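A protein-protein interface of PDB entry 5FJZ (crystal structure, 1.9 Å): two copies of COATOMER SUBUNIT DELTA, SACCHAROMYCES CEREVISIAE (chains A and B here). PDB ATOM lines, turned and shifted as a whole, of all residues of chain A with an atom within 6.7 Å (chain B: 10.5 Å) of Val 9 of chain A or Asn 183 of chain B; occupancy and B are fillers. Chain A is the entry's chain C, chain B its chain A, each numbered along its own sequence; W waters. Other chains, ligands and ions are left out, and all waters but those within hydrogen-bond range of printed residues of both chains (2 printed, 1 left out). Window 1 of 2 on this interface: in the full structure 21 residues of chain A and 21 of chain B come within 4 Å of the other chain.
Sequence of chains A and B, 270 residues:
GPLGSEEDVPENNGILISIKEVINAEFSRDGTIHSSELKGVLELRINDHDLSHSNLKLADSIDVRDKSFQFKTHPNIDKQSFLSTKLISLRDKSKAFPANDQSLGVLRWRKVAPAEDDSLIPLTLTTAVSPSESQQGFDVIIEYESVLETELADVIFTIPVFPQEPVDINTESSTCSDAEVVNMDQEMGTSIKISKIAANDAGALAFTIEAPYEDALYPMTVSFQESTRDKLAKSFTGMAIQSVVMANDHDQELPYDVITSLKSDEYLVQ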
ATOM      1  N   VAL A   9     -14.429 -27.123   3.606  1.00  0.00           N
ATOM      2  CA  VAL A   9     -15.133 -28.248   2.977  1.00  0.00           C
ATOM      3  C   VAL A   9     -14.117 -29.048   2.160  1.00  0.00           C
ATOM      4  O   VAL A   9     -13.633 -28.612   1.122  1.00  0.00           O
ATOM      5  CB  VAL A   9     -16.314 -27.798   2.100  1.00  0.00           C
ATOM      6  CG1 VAL A   9     -16.876 -28.950   1.273  1.00  0.00           C
ATOM      7  CG2 VAL A   9     -17.434 -27.261   2.972  1.00  0.00           C
ATOM      8  N   PRO A  10     -13.868 -30.282   2.567  1.00  0.00           N
ATOM      9  CA  PRO A  10     -12.982 -31.114   1.722  1.00  0.00           C
ATOM     10  C   PRO A  10     -13.517 -31.338   0.310  1.00  0.00           C
ATOM     11  O   PRO A  10     -14.743 -31.438   0.125  1.00  0.00           O
ATOM     12  CB  PRO A  10     -13.007 -32.492   2.423  1.00  0.00           C
ATOM     13  CG  PRO A  10     -13.638 -32.248   3.741  1.00  0.00           C
ATOM     14  CD  PRO A  10     -14.437 -31.023   3.691  1.00  0.00           C
ATOM     15  N   GLU A  11     -12.637 -31.450  -0.669  1.00  0.00           N
ATOM     16  CA  GLU A  11     -13.124 -31.667  -2.021  1.00  0.00           C
ATOM     17  C   GLU A  11     -13.526 -33.122  -2.205  1.00  0.00           C
ATOM     18  O   GLU A  11     -12.870 -34.042  -1.734  1.00  0.00           O
ATOM     19  CB  GLU A  11     -12.071 -31.253  -3.051  1.00  0.00           C
ATOM     20  CG  GLU A  11     -12.536 -31.435  -4.488  1.00  0.00           C
ATOM     21  CD  GLU A  11     -11.616 -30.792  -5.528  1.00  0.00           C
ATOM     22  OE1 GLU A  11     -10.513 -30.290  -5.168  1.00  0.00           O
ATOM     23  OE2 GLU A  11     -12.022 -30.816  -6.727  1.00  0.00           O
ATOM     24  N   ASN A  12     -14.573 -33.305  -2.983  1.00  0.00           N
ATOM     25  CA  ASN A  12     -15.054 -34.623  -3.436  1.00  0.00           C
ATOM     26  C   ASN A  12     -14.783 -34.752  -4.927  1.00  0.00           C
ATOM     27  O   ASN A  12     -15.158 -33.891  -5.680  1.00  0.00           O
ATOM     28  CB  ASN A  12     -16.560 -34.679  -3.171  1.00  0.00           C
ATOM     29  CG  ASN A  12     -17.217 -35.996  -3.518  1.00  0.00           C
ATOM     30  OD1 ASN A  12     -18.460 -36.137  -3.375  1.00  0.00           O
ATOM     31  ND2 ASN A  12     -16.471 -36.946  -3.851  1.00  0.00           N
ATOM     32  N   ARG A  45     -20.707 -38.800   0.526  1.00  0.00           N
ATOM     33  CA  ARG A  45     -20.976 -37.690  -0.385  1.00  0.00           C
ATOM     34  C   ARG A  45     -20.701 -38.183  -1.792  1.00  0.00           C
ATOM     35  O   ARG A  45     -19.626 -38.798  -2.085  1.00  0.00           O
ATOM     36  CB  ARG A  45     -20.085 -36.498  -0.153  1.00  0.00           C
ATOM     37  CG  ARG A  45     -20.466 -35.529   0.995  1.00  0.00           C
ATOM     38  CD  ARG A  45     -19.388 -34.528   1.299  1.00  0.00           C
ATOM     39  NE  ARG A  45     -19.016 -33.698   0.151  1.00  0.00           N
ATOM     40  CZ  ARG A  45     -17.937 -32.902   0.160  1.00  0.00           C
ATOM     41  NH1 ARG A  45     -17.149 -32.827   1.233  1.00  0.00           N
ATOM     42  NH2 ARG A  45     -17.661 -32.124  -0.895  1.00  0.00           N
ATOM     43  N   ASN A 100     -25.954 -34.944  -5.514  1.00  0.00           N
ATOM     44  CA  ASN A 100     -25.579 -33.563  -5.572  1.00  0.00           C
ATOM     45  C   ASN A 100     -24.705 -33.073  -4.403  1.00  0.00           C
ATOM     46  O   ASN A 100     -24.933 -32.017  -3.811  1.00  0.00           O
ATOM     47  CB  ASN A 100     -26.855 -32.679  -5.699  1.00  0.00           C
ATOM     48  CG  ASN A 100     -27.518 -32.792  -7.094  1.00  0.00           C
ATOM     49  OD1 ASN A 100     -26.965 -32.352  -8.108  1.00  0.00           O
ATOM     50  ND2 ASN A 100     -28.611 -33.435  -7.141  1.00  0.00           N
ATOM     51  N   ASP A 101     -23.694 -33.876  -4.091  1.00  0.00           N
ATOM     52  CA  ASP A 101     -22.749 -33.621  -3.053  1.00  0.00           C
ATOM     53  C   ASP A 101     -23.316 -33.337  -1.670  1.00  0.00           C
ATOM     54  O   ASP A 101     -22.711 -32.588  -0.927  1.00  0.00           O
ATOM     55  CB  ASP A 101     -21.777 -32.513  -3.486  1.00  0.00           C
ATOM     56  CG  ASP A 101     -20.336 -32.787  -3.061  1.00  0.00           C
ATOM     57  OD1 ASP A 101     -20.061 -33.893  -2.504  1.00  0.00           O
ATOM     58  OD2 ASP A 101     -19.444 -31.908  -3.260  1.00  0.00           O
ATOM     59  N   GLN A 102     -24.429 -33.938  -1.321  1.00  0.00           N
ATOM     60  CA  GLN A 102     -24.994 -33.827   0.012  1.00  0.00           C
ATOM     61  C   GLN A 102     -24.347 -34.823   0.931  1.00  0.00           C
ATOM     62  O   GLN A 102     -24.088 -35.976   0.530  1.00  0.00           O
ATOM     63  CB  GLN A 102     -26.514 -34.072   0.007  1.00  0.00           C
ATOM     64  CG  GLN A 102     -27.285 -33.248  -1.065  1.00  0.00           C
ATOM     65  CD  GLN A 102     -27.595 -33.995  -2.344  1.00  0.00           C
ATOM     66  OE1 GLN A 102     -26.851 -34.905  -2.763  1.00  0.00           O
ATOM     67  NE2 GLN A 102     -28.727 -33.687  -2.943  1.00  0.00           N
ATOM     68  N   SER A 103     -24.103 -34.392   2.172  1.00  0.00           N
ATOM     69  CA  SER A 103     -23.537 -35.296   3.177  1.00  0.00           C
ATOM     70  C   SER A 103     -24.658 -36.228   3.682  1.00  0.00           C
ATOM     71  O   SER A 103     -25.618 -35.784   4.319  1.00  0.00           O
ATOM     72  CB  SER A 103     -22.925 -34.538   4.337  1.00  0.00           C
ATOM     73  OG  SER A 103     -21.842 -33.755   3.953  1.00  0.00           O
ATOM     74  N   LEU A 104     -24.531 -37.508   3.375  1.00  0.00           N
ATOM     75  CA  LEU A 104     -25.510 -38.494   3.712  1.00  0.00           C
ATOM     76  C   LEU A 104     -24.978 -39.328   4.881  1.00  0.00           C
ATOM     77  O   LEU A 104     -24.076 -40.139   4.670  1.00  0.00           O
ATOM     78  CB  LEU A 104     -25.817 -39.372   2.534  1.00  0.00           C
ATOM     79  CG  LEU A 104     -26.106 -38.649   1.197  1.00  0.00           C
ATOM     80  CD1 LEU A 104     -26.218 -39.654   0.085  1.00  0.00           C
ATOM     81  CD2 LEU A 104     -27.387 -37.775   1.245  1.00  0.00           C
ATOM     82  N   ASP B 154     -19.528 -15.771  -2.477  1.00  0.00           N
ATOM     83  CA  ASP B 154     -19.870 -17.153  -2.067  1.00  0.00           C
ATOM     84  C   ASP B 154     -21.158 -17.245  -1.293  1.00  0.00           C
ATOM     85  O   ASP B 154     -21.227 -17.840  -0.183  1.00  0.00           O
ATOM     86  CB  ASP B 154     -18.687 -17.764  -1.242  1.00  0.00           C
ATOM     87  CG  ASP B 154     -17.401 -17.908  -2.076  1.00  0.00           C
ATOM     88  OD1 ASP B 154     -17.473 -17.997  -3.311  1.00  0.00           O
ATOM     89  OD2 ASP B 154     -16.308 -17.947  -1.494  1.00  0.00           O
ATOM     90  N   VAL B 155     -22.236 -16.769  -1.891  1.00  0.00           N
ATOM     91  CA  VAL B 155     -23.604 -16.861  -1.350  1.00  0.00           C
ATOM     92  C   VAL B 155     -24.242 -18.214  -1.729  1.00  0.00           C
ATOM     93  O   VAL B 155     -24.150 -18.670  -2.861  1.00  0.00           O
ATOM     94  CB  VAL B 155     -24.428 -15.743  -1.923  1.00  0.00           C
ATOM     95  CG1 VAL B 155     -25.874 -15.730  -1.416  1.00  0.00           C
ATOM     96  CG2 VAL B 155     -23.745 -14.411  -1.659  1.00  0.00           C
ATOM     97  N   ILE B 156     -24.817 -18.873  -0.754  1.00  0.00           N
ATOM     98  CA  ILE B 156     -25.301 -20.221  -0.877  1.00  0.00           C
ATOM     99  C   ILE B 156     -26.804 -20.282  -0.698  1.00  0.00           C
ATOM    100  O   ILE B 156     -27.385 -19.800   0.308  1.00  0.00           O
ATOM    101  CB  ILE B 156     -24.569 -21.159   0.083  1.00  0.00           C
ATOM    102  CG1 ILE B 156     -23.082 -21.147  -0.316  1.00  0.00           C
ATOM    103  CG2 ILE B 156     -25.096 -22.569  -0.086  1.00  0.00           C
ATOM    104  CD1 ILE B 156     -22.194 -21.958   0.591  1.00  0.00           C
ATOM    105  N   PHE B 157     -27.464 -20.827  -1.710  1.00  0.00           N
ATOM    106  CA  PHE B 157     -28.908 -21.123  -1.632  1.00  0.00           C
ATOM    107  C   PHE B 157     -29.175 -22.605  -1.413  1.00  0.00           C
ATOM    108  O   PHE B 157     -28.572 -23.457  -2.115  1.00  0.00           O
ATOM    109  CB  PHE B 157     -29.585 -20.658  -2.950  1.00  0.00           C
ATOM    110  CG  PHE B 157     -29.362 -19.210  -3.249  1.00  0.00           C
ATOM    111  CD1 PHE B 157     -28.175 -18.812  -3.909  1.00  0.00           C
ATOM    112  CD2 PHE B 157     -30.304 -18.282  -2.950  1.00  0.00           C
ATOM    113  CE1 PHE B 157     -27.930 -17.461  -4.143  1.00  0.00           C
ATOM    114  CE2 PHE B 157     -30.092 -16.940  -3.173  1.00  0.00           C
ATOM    115  CZ  PHE B 157     -28.912 -16.543  -3.814  1.00  0.00           C
ATOM    116  N   THR B 158     -30.008 -22.922  -0.449  1.00  0.00           N
ATOM    117  CA  THR B 158     -30.289 -24.331  -0.087  1.00  0.00           C
ATOM    118  C   THR B 158     -31.770 -24.613  -0.300  1.00  0.00           C
ATOM    119  O   THR B 158     -32.631 -23.906   0.154  1.00  0.00           O
ATOM    120  CB  THR B 158     -29.806 -24.699   1.351  1.00  0.00           C
ATOM    121  OG1 THR B 158     -28.409 -24.460   1.324  1.00  0.00           O
ATOM    122  CG2 THR B 158     -30.118 -26.164   1.654  1.00  0.00           C
ATOM    123  N   PHE B 162     -33.642 -33.795  -1.822  1.00  0.00           N
ATOM    124  CA  PHE B 162     -32.447 -34.574  -2.149  1.00  0.00           C
ATOM    125  C   PHE B 162     -32.743 -35.355  -3.441  1.00  0.00           C
ATOM    126  O   PHE B 162     -33.258 -36.481  -3.353  1.00  0.00           O
ATOM    127  CB  PHE B 162     -32.174 -35.637  -1.034  1.00  0.00           C
ATOM    128  CG  PHE B 162     -31.791 -35.038   0.296  1.00  0.00           C
ATOM    129  CD1 PHE B 162     -32.767 -34.516   1.110  1.00  0.00           C
ATOM    130  CD2 PHE B 162     -30.495 -34.882   0.638  1.00  0.00           C
ATOM    131  CE1 PHE B 162     -32.435 -33.881   2.297  1.00  0.00           C
ATOM    132  CE2 PHE B 162     -30.138 -34.221   1.796  1.00  0.00           C
ATOM    133  CZ  PHE B 162     -31.112 -33.737   2.636  1.00  0.00           C
ATOM    134  N   GLU B 180     -22.796 -23.226  -8.928  1.00  0.00           N
ATOM    135  CA  GLU B 180     -22.505 -24.643  -8.876  1.00  0.00           C
ATOM    136  C   GLU B 180     -23.048 -25.255  -7.583  1.00  0.00           C
ATOM    137  O   GLU B 180     -23.076 -24.593  -6.580  1.00  0.00           O
ATOM    138  CB  GLU B 180     -20.974 -24.905  -8.972  1.00  0.00           C
ATOM    139  CG  GLU B 180     -20.207 -24.428  -7.765  1.00  0.00           C
ATOM    140  CD  GLU B 180     -18.687 -24.366  -7.945  1.00  0.00           C
ATOM    141  OE1 GLU B 180     -18.145 -25.086  -8.788  1.00  0.00           O
ATOM    142  OE2 GLU B 180     -18.029 -23.614  -7.186  1.00  0.00           O
ATOM    143  N   VAL B 181     -23.404 -26.533  -7.645  1.00  0.00           N
ATOM    144  CA  VAL B 181     -23.763 -27.225  -6.440  1.00  0.00           C
ATOM    145  C   VAL B 181     -22.525 -27.354  -5.576  1.00  0.00           C
ATOM    146  O   VAL B 181     -21.394 -27.573  -6.089  1.00  0.00           O
ATOM    147  CB  VAL B 181     -24.677 -28.450  -6.622  1.00  0.00           C
ATOM    148  CG1 VAL B 181     -25.139 -28.677  -8.038  1.00  0.00           C
ATOM    149  CG2 VAL B 181     -24.237 -29.665  -5.855  1.00  0.00           C
ATOM    150  N   VAL B 182     -22.732 -27.233  -4.276  1.00  0.00           N
ATOM    151  CA  VAL B 182     -21.684 -27.340  -3.273  1.00  0.00           C
ATOM    152  C   VAL B 182     -22.186 -28.125  -2.079  1.00  0.00           C
ATOM    153  O   VAL B 182     -23.384 -28.216  -1.824  1.00  0.00           O
ATOM    154  CB  VAL B 182     -21.155 -25.954  -2.760  1.00  0.00           C
ATOM    155  CG1 VAL B 182     -20.410 -25.215  -3.872  1.00  0.00           C
ATOM    156  CG2 VAL B 182     -22.245 -25.182  -2.173  1.00  0.00           C
ATOM    157  N   ASN B 183     -21.233 -28.721  -1.352  1.00  0.00           N
ATOM    158  CA  ASN B 183     -21.589 -29.353  -0.152  1.00  0.00           C
ATOM    159  C   ASN B 183     -21.638 -28.230   0.924  1.00  0.00           C
ATOM    160  O   ASN B 183     -20.704 -27.517   1.087  1.00  0.00           O
ATOM    161  CB  ASN B 183     -20.575 -30.405   0.229  1.00  0.00           C
ATOM    162  CG  ASN B 183     -20.866 -31.001   1.595  1.00  0.00           C
ATOM    163  OD1 ASN B 183     -20.079 -30.804   2.533  1.00  0.00           O
ATOM    164  ND2 ASN B 183     -21.865 -31.876   1.670  1.00  0.00           N
ATOM    165  N   MET B 184     -22.690 -28.207   1.689  1.00  0.00           N
ATOM    166  CA  MET B 184     -22.887 -27.220   2.699  1.00  0.00           C
ATOM    167  C   MET B 184     -23.724 -27.927   3.745  1.00  0.00           C
ATOM    168  O   MET B 184     -24.950 -27.991   3.677  1.00  0.00           O
ATOM    169  CB  MET B 184     -23.565 -26.038   2.039  1.00  0.00           C
ATOM    170  CG  MET B 184     -24.620 -25.327   2.822  1.00  0.00           C
ATOM    171  SD  MET B 184     -23.778 -24.297   3.998  1.00  0.00           S
ATOM    172  CE  MET B 184     -25.034 -23.060   4.141  1.00  0.00           C
ATOM    173  N   ASP B 185     -23.093 -28.446   4.781  1.00  0.00           N
ATOM    174  CA  ASP B 185     -23.961 -29.210   5.670  1.00  0.00           C
ATOM    175  C   ASP B 185     -24.580 -28.468   6.894  1.00  0.00           C
ATOM    176  O   ASP B 185     -25.299 -29.089   7.647  1.00  0.00           O
ATOM    177  CB  ASP B 185     -23.382 -30.582   5.973  1.00  0.00           C
ATOM    178  CG  ASP B 185     -22.056 -30.494   6.540  1.00  0.00           C
ATOM    179  OD1 ASP B 185     -21.825 -29.458   7.164  1.00  0.00           O
ATOM    180  OD2 ASP B 185     -21.298 -31.469   6.420  1.00  0.00           O
ATOM    181  N   GLN B 186     -24.370 -27.157   6.991  1.00  0.00           N
ATOM    182  CA  GLN B 186     -25.081 -26.266   7.945  1.00  0.00           C
ATOM    183  C   GLN B 186     -26.586 -26.134   7.599  1.00  0.00           C
ATOM    184  O   GLN B 186     -27.344 -25.636   8.394  1.00  0.00           O
ATOM    185  CB  GLN B 186     -24.490 -24.838   7.913  1.00  0.00           C
ATOM    186  CG  GLN B 186     -23.144 -24.690   8.593  1.00  0.00           C
ATOM    187  CD  GLN B 186     -22.041 -25.398   7.816  1.00  0.00           C
ATOM    188  OE1 GLN B 186     -21.705 -25.001   6.693  1.00  0.00           O
ATOM    189  NE2 GLN B 186     -21.470 -26.455   8.402  1.00  0.00           N
ATOM    190  N   GLU B 187     -26.999 -26.480   6.379  1.00  0.00           N
ATOM    191  CA  GLU B 187     -28.405 -26.468   6.015  1.00  0.00           C
ATOM    192  C   GLU B 187     -28.738 -27.787   5.368  1.00  0.00           C
ATOM    193  O   GLU B 187     -27.921 -28.385   4.667  1.00  0.00           O
ATOM    194  CB  GLU B 187     -28.764 -25.309   5.049  1.00  0.00           C
ATOM    195  CG  GLU B 187     -28.542 -23.900   5.602  1.00  0.00           C
ATOM    196  CD  GLU B 187     -29.356 -23.564   6.869  1.00  0.00           C
ATOM    197  OE1 GLU B 187     -30.385 -24.252   7.162  1.00  0.00           O
ATOM    198  OE2 GLU B 187     -28.934 -22.591   7.586  1.00  0.00           O
ATOM    199  N   MET B 188     -29.933 -28.248   5.580  1.00  0.00           N
ATOM    200  CA  MET B 188     -30.352 -29.499   5.041  1.00  0.00           C
ATOM    201  C   MET B 188     -30.878 -29.378   3.592  1.00  0.00           C
ATOM    202  O   MET B 188     -31.812 -28.621   3.320  1.00  0.00           O
ATOM    203  CB  MET B 188     -31.484 -30.018   5.887  1.00  0.00           C
ATOM    204  CG  MET B 188     -31.955 -31.411   5.458  1.00  0.00           C
ATOM    205  SD  MET B 188     -33.703 -31.683   5.772  1.00  0.00           S
ATOM    206  CE  MET B 188     -33.804 -31.222   7.527  1.00  0.00           C
ATOM    207  N   GLY B 189     -30.367 -30.236   2.711  1.00  0.00           N
ATOM    208  CA  GLY B 189     -30.905 -30.353   1.324  1.00  0.00           C
ATOM    209  C   GLY B 189     -29.783 -30.145   0.351  1.00  0.00           C
ATOM    210  O   GLY B 189     -28.640 -30.502   0.609  1.00  0.00           O
ATOM    211  N   THR B 190     -30.128 -29.582  -0.796  1.00  0.00           N
ATOM    212  CA  THR B 190     -29.200 -29.382  -1.888  1.00  0.00           C
ATOM    213  C   THR B 190     -28.799 -27.899  -1.991  1.00  0.00           C
ATOM    214  O   THR B 190     -29.640 -27.034  -1.989  1.00  0.00           O
ATOM    215  CB  THR B 190     -29.885 -29.860  -3.173  1.00  0.00           C
ATOM    216  OG1 THR B 190     -30.326 -31.222  -2.986  1.00  0.00           O
ATOM    217  CG2 THR B 190     -28.945 -29.722  -4.367  1.00  0.00           C
ATOM    218  N   SER B 191     -27.506 -27.634  -2.087  1.00  0.00           N
ATOM    219  CA  SER B 191     -26.955 -26.300  -1.953  1.00  0.00           C
ATOM    220  C   SER B 191     -26.249 -25.868  -3.233  1.00  0.00           C
ATOM    221  O   SER B 191     -25.416 -26.607  -3.803  1.00  0.00           O
ATOM    222  CB  SER B 191     -25.977 -26.161  -0.799  1.00  0.00           C
ATOM    223  OG  SER B 191     -26.669 -26.339   0.442  1.00  0.00           O
ATOM    224  N   ILE B 192     -26.542 -24.648  -3.639  1.00  0.00           N
ATOM    225  CA  ILE B 192     -25.973 -24.022  -4.860  1.00  0.00           C
ATOM    226  C   ILE B 192     -25.312 -22.748  -4.471  1.00  0.00           C
ATOM    227  O   ILE B 192     -25.918 -21.871  -3.845  1.00  0.00           O
ATOM    228  CB  ILE B 192     -27.055 -23.709  -5.970  1.00  0.00           C
ATOM    229  CG1 ILE B 192     -27.762 -24.983  -6.348  1.00  0.00           C
ATOM    230  CG2 ILE B 192     -26.315 -23.025  -7.144  1.00  0.00           C
ATOM    231  CD1 ILE B 192     -29.094 -24.774  -7.110  1.00  0.00           C
ATOM    232  N   LYS B 193     -24.075 -22.583  -4.882  1.00  0.00           N
ATOM    233  CA  LYS B 193     -23.342 -21.417  -4.567  1.00  0.00           C
ATOM    234  C   LYS B 193     -23.205 -20.538  -5.727  1.00  0.00           C
ATOM    235  O   LYS B 193     -22.883 -20.998  -6.817  1.00  0.00           O
ATOM    236  CB  LYS B 193     -21.943 -21.809  -4.148  1.00  0.00           C
ATOM    237  CG  LYS B 193     -20.969 -20.682  -3.849  1.00  0.00           C
ATOM    238  CD  LYS B 193     -19.852 -21.114  -2.868  1.00  0.00           C
ATOM    239  CE  LYS B 193     -18.518 -21.266  -3.537  1.00  0.00           C
ATOM    240  NZ  LYS B 193     -18.489 -22.224  -4.652  1.00  0.00           N
ATOM    241  N   SER B 223     -27.489 -18.332   2.628  1.00  0.00           N
ATOM    242  CA  SER B 223     -26.364 -18.218   3.547  1.00  0.00           C
ATOM    243  C   SER B 223     -25.313 -17.293   2.952  1.00  0.00           C
ATOM    244  O   SER B 223     -24.839 -17.539   1.815  1.00  0.00           O
ATOM    245  CB  SER B 223     -25.795 -19.639   3.766  1.00  0.00           C
ATOM    246  OG  SER B 223     -24.705 -19.635   4.686  1.00  0.00           O
HETATM  247  O   HOH W   1     -25.030 -31.858   2.914  1.00  0.00           O
HETATM  248  O   HOH W   2     -25.433 -29.890  -2.056  1.00  0.00           O
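The side-chain amide nitrogen (ND2) of Asn 183 of chain B sits at hydrogen-bond distance from the side-chain hydroxyl (OG) of Ser 103 of chain A. The side-chain carboxylate (OD2) of Asp 185 of chain B lies within hydrogen-bond range of the side-chain hydroxyl (OG) of Ser 103 of chain A, at 3.4 Å. The side-chain amide nitrogen (NE2) of Gln 102 of chain A lies within hydrogen-bond range of the side-chain hydroxyl (OG1) of Thr 190 of chain B (2.9 Å). O of Asp 101 of chain A lies within hydrogen-bond range of ND2 of Asn 183 of chain B (2.8 Å).
The side-chain amide oxygen (OD1) of Asn 12 of chain A lies close to the side-chain carboxylate (OD1) of Asp 101 of chain A (2.9 Å). The guanidinium group (NE) of Arg 45 of chain A is in salt-bridge range of the side-chain carboxylate (OD1) of Asp 101 of chain A (2.9 Å). The backbone NH (N) of Asn 100 of chain A sits at hydrogen-bond distance from the side-chain amide oxygen (OE1) of Gln 102 of chain A (2.9 Å). OD1 of Asn 12 of chain A sits close to O of Arg 45 of chain A (3.2 Å). The side-chain amide nitrogen (NE2) of Gln 186 of chain B is in hydrogen-bond range of the side-chain carboxylate (OD1) of Asp 185 of chain B. NH1 of Arg 45 of chain A is in hydrogen-bond range of O of Pro 10 of chain A, 3.0 Å away.
Val 9 of chain A touches Asn 183 of chain B (CG2 to O, 3.8 Å). CB of Asn 183 of chain B touches NH2 of Arg 45 of chain A, 3.6 Å away. Val 181 of chain B touches Asn 100 of chain A. Asn 100 of chain A touches Thr 190 of chain B (CB to CG2, 3.9 Å). Gln 102 of chain A touches Phe 162 of chain B (NE2 to CA, 3.9 Å). ND2 of Asn 183 of chain B touches C of Gln 102 of chain A, at 3.9 Å. CG of Gln 102 of chain A touches O of Gly 189 of chain B (3.5 Å).
Printed residues of chain B within 4 Å of Val 9 of chain A: Asn 183 (3.8 Å). No residue of chain B comes within 4 Å of Pro 10 of chain A. Printed residues of chain B within 4 Å of Arg 45 of chain A: Asn 183. Of chain B, only Asn 183 and Asp 185 come within 4 Å of Ser 103 of chain A. Of the printed residues of chain A, Phe 162 of chain B touches Gln 102. Asn 183 of chain B touches just these residues of chain A: Val 9, Arg 45, Asp 101, Gln 102 and Ser 103. Of the printed residues of chain A, Thr 190 of chain B touches Asn 100 (3.9 Å) and Gln 102 (2.9 Å). The nearest residue of chain B that does not touch Val 9 of chain A is Met 184 of chain B (5.5 Å). The nearest residue of chain A that does not touch Asn 183 of chain B is Asn 100 of chain A (5.5 Å).
Of the 21 printed residues of chain B, 6 touch a printed residue of chain A. Printed residues of chain B that touch a printed residue of chain A: Phe 162, Val 181, Asn 183, Asp 185, Gly 189 and Thr 190. Hydrophobic or aromatic side chains of chain B within 4 Å of the printed part of chain A: Phe 162 and Val 181. Along chain B the printed residues that touch a printed residue of chain A span positions 162 to 190. Of the 10 printed residues of chain A, 6 touch a printed residue of chain B.
No position is printed for both chains.
Water W2 lies within hydrogen-bond range of O of Val 182 of chain B, O of Asn 100 of chain A and N of Ser 191 of chain B. Water W1 lies within hydrogen-bond range of N of Ser 103 of chain A and ND2 of Asn 183 of chain B.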
